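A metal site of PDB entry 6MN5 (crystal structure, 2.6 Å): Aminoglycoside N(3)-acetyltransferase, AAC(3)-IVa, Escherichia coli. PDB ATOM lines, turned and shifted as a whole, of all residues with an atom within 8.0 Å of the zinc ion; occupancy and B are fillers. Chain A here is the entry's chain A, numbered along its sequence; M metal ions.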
ATOM      1  N   HIS A 192      22.301   9.516   8.800  1.00  0.00           N
ATOM      2  CA  HIS A 192      22.584   8.106   8.627  1.00  0.00           C
ATOM      3  C   HIS A 192      23.028   7.527   9.969  1.00  0.00           C
ATOM      4  O   HIS A 192      22.628   8.034  11.023  1.00  0.00           O
ATOM      5  CB  HIS A 192      23.655   7.885   7.548  1.00  0.00           C
ATOM      6  CG  HIS A 192      24.762   8.890   7.602  1.00  0.00           C
ATOM      7  ND1 HIS A 192      25.849   8.748   8.434  1.00  0.00           N
ATOM      8  CD2 HIS A 192      24.957  10.050   6.932  1.00  0.00           C
ATOM      9  CE1 HIS A 192      26.661   9.782   8.273  1.00  0.00           C
ATOM     10  NE2 HIS A 192      26.141  10.581   7.361  1.00  0.00           N
ATOM     11  N   CYS A 193      23.855   6.479   9.953  1.00  0.00           N
ATOM     12  CA  CYS A 193      24.283   5.839  11.192  1.00  0.00           C
ATOM     13  C   CYS A 193      25.441   6.556  11.865  1.00  0.00           C
ATOM     14  O   CYS A 193      25.699   6.308  13.040  1.00  0.00           O
ATOM     15  CB  CYS A 193      24.653   4.385  10.927  1.00  0.00           C
ATOM     16  SG  CYS A 193      26.275   4.178  10.161  1.00  0.00           S
ATOM     17  N   CYS A 194      26.147   7.426  11.140  1.00  0.00           N
ATOM     18  CA  CYS A 194      27.265   8.242  11.629  1.00  0.00           C
ATOM     19  C   CYS A 194      28.492   7.434  12.008  1.00  0.00           C
ATOM     20  O   CYS A 194      29.475   8.014  12.489  1.00  0.00           O
ATOM     21  CB  CYS A 194      26.875   9.115  12.829  1.00  0.00           C
ATOM     22  SG  CYS A 194      25.524  10.271  12.550  1.00  0.00           S
ATOM     23  N   GLU A 195      28.491   6.104  11.808  1.00  0.00           N
ATOM     24  CA  GLU A 195      29.648   5.302  12.189  1.00  0.00           C
ATOM     25  C   GLU A 195      30.883   5.682  11.380  1.00  0.00           C
ATOM     26  O   GLU A 195      31.991   5.757  11.931  1.00  0.00           O
ATOM     27  CB  GLU A 195      29.338   3.811  12.003  1.00  0.00           C
ATOM     28  CG  GLU A 195      28.575   3.184  13.164  1.00  0.00           C
ATOM     29  CD  GLU A 195      28.346   1.707  12.968  1.00  0.00           C
ATOM     30  OE1 GLU A 195      29.101   1.082  12.190  1.00  0.00           O
ATOM     31  OE2 GLU A 195      27.408   1.163  13.583  1.00  0.00           O
ATOM     32  N   ARG A 196      30.723   5.928  10.084  1.00  0.00           N
ATOM     33  CA  ARG A 196      31.860   6.233   9.225  1.00  0.00           C
ATOM     34  C   ARG A 196      32.362   7.657   9.398  1.00  0.00           C
ATOM     35  O   ARG A 196      33.293   8.049   8.687  1.00  0.00           O
ATOM     36  CB  ARG A 196      31.493   5.974   7.768  1.00  0.00           C
ATOM     37  CG  ARG A 196      31.391   4.494   7.420  1.00  0.00           C
ATOM     38  CD  ARG A 196      30.812   4.270   6.045  1.00  0.00           C
ATOM     39  NE  ARG A 196      31.634   4.875   4.997  1.00  0.00           N
ATOM     40  CZ  ARG A 196      32.654   4.268   4.409  1.00  0.00           C
ATOM     41  NH1 ARG A 196      32.972   3.027   4.768  1.00  0.00           N
ATOM     42  NH2 ARG A 196      33.352   4.889   3.471  1.00  0.00           N
ATOM     43  N   PHE A 243      30.497   8.805   3.702  1.00  0.00           N
ATOM     44  CA  PHE A 243      30.064   8.531   5.071  1.00  0.00           C
ATOM     45  C   PHE A 243      29.003   7.448   5.170  1.00  0.00           C
ATOM     46  O   PHE A 243      28.688   7.010   6.278  1.00  0.00           O
ATOM     47  CB  PHE A 243      29.529   9.820   5.716  1.00  0.00           C
ATOM     48  CG  PHE A 243      30.604  10.808   6.095  1.00  0.00           C
ATOM     49  CD1 PHE A 243      31.827  10.366   6.580  1.00  0.00           C
ATOM     50  CD2 PHE A 243      30.400  12.164   5.944  1.00  0.00           C
ATOM     51  CE1 PHE A 243      32.823  11.273   6.916  1.00  0.00           C
ATOM     52  CE2 PHE A 243      31.390  13.078   6.277  1.00  0.00           C
ATOM     53  CZ  PHE A 243      32.602  12.629   6.769  1.00  0.00           C
ATOM     54  N   LEU A 244      28.455   7.000   4.043  1.00  0.00           N
ATOM     55  CA  LEU A 244      27.419   5.970   4.042  1.00  0.00           C
ATOM     56  C   LEU A 244      28.035   4.594   3.881  1.00  0.00           C
ATOM     57  O   LEU A 244      28.957   4.396   3.075  1.00  0.00           O
ATOM     58  CB  LEU A 244      26.398   6.216   2.942  1.00  0.00           C
ATOM     59  CG  LEU A 244      25.890   7.643   2.723  1.00  0.00           C
ATOM     60  CD1 LEU A 244      24.906   7.667   1.570  1.00  0.00           C
ATOM     61  CD2 LEU A 244      25.258   8.182   3.992  1.00  0.00           C
ATOM     62  N   HIS A 245      27.515   3.631   4.645  1.00  0.00           N
ATOM     63  CA  HIS A 245      27.952   2.253   4.504  1.00  0.00           C
ATOM     64  C   HIS A 245      27.655   1.756   3.084  1.00  0.00           C
ATOM     65  O   HIS A 245      26.695   2.197   2.451  1.00  0.00           O
ATOM     66  CB  HIS A 245      27.257   1.367   5.528  1.00  0.00           C
ATOM     67  CG  HIS A 245      27.942   1.322   6.859  1.00  0.00           C
ATOM     68  ND1 HIS A 245      27.515   2.063   7.938  1.00  0.00           N
ATOM     69  CD2 HIS A 245      29.027   0.641   7.271  1.00  0.00           C
ATOM     70  CE1 HIS A 245      28.310   1.833   8.973  1.00  0.00           C
ATOM     71  NE2 HIS A 245      29.241   0.971   8.594  1.00  0.00           N
ATOM     72  N   PRO A 246      28.468   0.837   2.569  1.00  0.00           N
ATOM     73  CA  PRO A 246      28.123   0.189   1.308  1.00  0.00           C
ATOM     74  C   PRO A 246      26.886  -0.668   1.476  1.00  0.00           C
ATOM     75  O   PRO A 246      26.567  -1.105   2.594  1.00  0.00           O
ATOM     76  CB  PRO A 246      29.366  -0.671   1.008  1.00  0.00           C
ATOM     77  CG  PRO A 246      30.021  -0.865   2.331  1.00  0.00           C
ATOM     78  CD  PRO A 246      29.765   0.384   3.098  1.00  0.00           C
ATOM     79  N   ALA A 249      27.108  -3.785   3.529  1.00  0.00           N
ATOM     80  CA  ALA A 249      27.151  -3.695   4.982  1.00  0.00           C
ATOM     81  C   ALA A 249      25.784  -3.942   5.621  1.00  0.00           C
ATOM     82  O   ALA A 249      25.724  -4.323   6.794  1.00  0.00           O
ATOM     83  CB  ALA A 249      27.667  -2.318   5.413  1.00  0.00           C
ATOM     84  N   GLY A 250      24.696  -3.733   4.874  1.00  0.00           N
ATOM     85  CA  GLY A 250      23.372  -3.955   5.411  1.00  0.00           C
ATOM     86  C   GLY A 250      22.939  -2.967   6.469  1.00  0.00           C
ATOM     87  O   GLY A 250      22.025  -3.272   7.239  1.00  0.00           O
ATOM     88  N   CYS A 251      23.560  -1.787   6.526  1.00  0.00           N
ATOM     89  CA  CYS A 251      23.140  -0.774   7.480  1.00  0.00           C
ATOM     90  C   CYS A 251      21.812  -0.170   7.031  1.00  0.00           C
ATOM     91  O   CYS A 251      21.722   0.396   5.941  1.00  0.00           O
ATOM     92  CB  CYS A 251      24.193   0.317   7.617  1.00  0.00           C
ATOM     93  SG  CYS A 251      23.585   1.817   8.432  1.00  0.00           S
ATOM     94  N   GLU A 252      20.796  -0.290   7.883  1.00  0.00           N
ATOM     95  CA  GLU A 252      19.451   0.162   7.519  1.00  0.00           C
ATOM     96  C   GLU A 252      19.433   1.659   7.248  1.00  0.00           C
ATOM     97  O   GLU A 252      18.866   2.107   6.239  1.00  0.00           O
ATOM     98  CB  GLU A 252      18.478  -0.187   8.646  1.00  0.00           C
ATOM     99  CG  GLU A 252      17.125  -0.695   8.178  1.00  0.00           C
ATOM    100  CD  GLU A 252      16.386  -1.430   9.275  1.00  0.00           C
ATOM    101  OE1 GLU A 252      16.432  -2.674   9.300  1.00  0.00           O
ATOM    102  OE2 GLU A 252      15.756  -0.758  10.117  1.00  0.00           O
ATOM    103  N   GLU A 253      20.048   2.453   8.121  1.00  0.00           N
ATOM    104  CA  GLU A 253      19.947   3.898   8.011  1.00  0.00           C
ATOM    105  C   GLU A 253      20.708   4.431   6.809  1.00  0.00           C
ATOM    106  O   GLU A 253      20.204   5.302   6.086  1.00  0.00           O
ATOM    107  CB  GLU A 253      20.444   4.556   9.295  1.00  0.00           C
ATOM    108  CG  GLU A 253      19.981   3.852  10.554  1.00  0.00           C
ATOM    109  CD  GLU A 253      20.564   4.475  11.800  1.00  0.00           C
ATOM    110  OE1 GLU A 253      20.440   5.711  11.959  1.00  0.00           O
ATOM    111  OE2 GLU A 253      21.142   3.738  12.626  1.00  0.00           O
ATOM    112  N   CYS A 254      21.932   3.934   6.578  1.00  0.00           N
ATOM    113  CA  CYS A 254      22.674   4.341   5.393  1.00  0.00           C
ATOM    114  C   CYS A 254      21.972   3.871   4.124  1.00  0.00           C
ATOM    115  O   CYS A 254      21.985   4.583   3.106  1.00  0.00           O
ATOM    116  CB  CYS A 254      24.097   3.787   5.456  1.00  0.00           C
ATOM    117  SG  CYS A 254      25.136   4.560   6.707  1.00  0.00           S
ATOM    118  N   ASP A 255      21.347   2.701   4.163  1.00  0.00           N
ATOM    119  CA  ASP A 255      20.559   2.248   3.021  1.00  0.00           C
ATOM    120  C   ASP A 255      19.406   3.216   2.745  1.00  0.00           C
ATOM    121  O   ASP A 255      19.115   3.514   1.588  1.00  0.00           O
ATOM    122  CB  ASP A 255      20.016   0.840   3.265  1.00  0.00           C
ATOM    123  CG  ASP A 255      21.083  -0.231   3.104  1.00  0.00           C
ATOM    124  OD1 ASP A 255      22.241   0.132   2.818  1.00  0.00           O
ATOM    125  OD2 ASP A 255      20.754  -1.419   3.281  1.00  0.00           O
HETATM  126 ZN    ZN M   1      25.588   2.881   8.347  1.00  0.00          ZN
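SG of Cys 251 lies close to N of Glu 253. SG of Cys 193 sits close to N of Glu 195, at 3.4 Å.
Of the 16 residues printed, 4 come within 4 Å of the zinc ion.
The zinc ion is bound by ND1 of His 245 (2.1 Å), SG of Cys 251 (2.3 Å), SG of Cys 193 (2.3 Å) and SG of Cys 254 (2.4 Å). The zinc ion has four donor atoms within binding distance.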
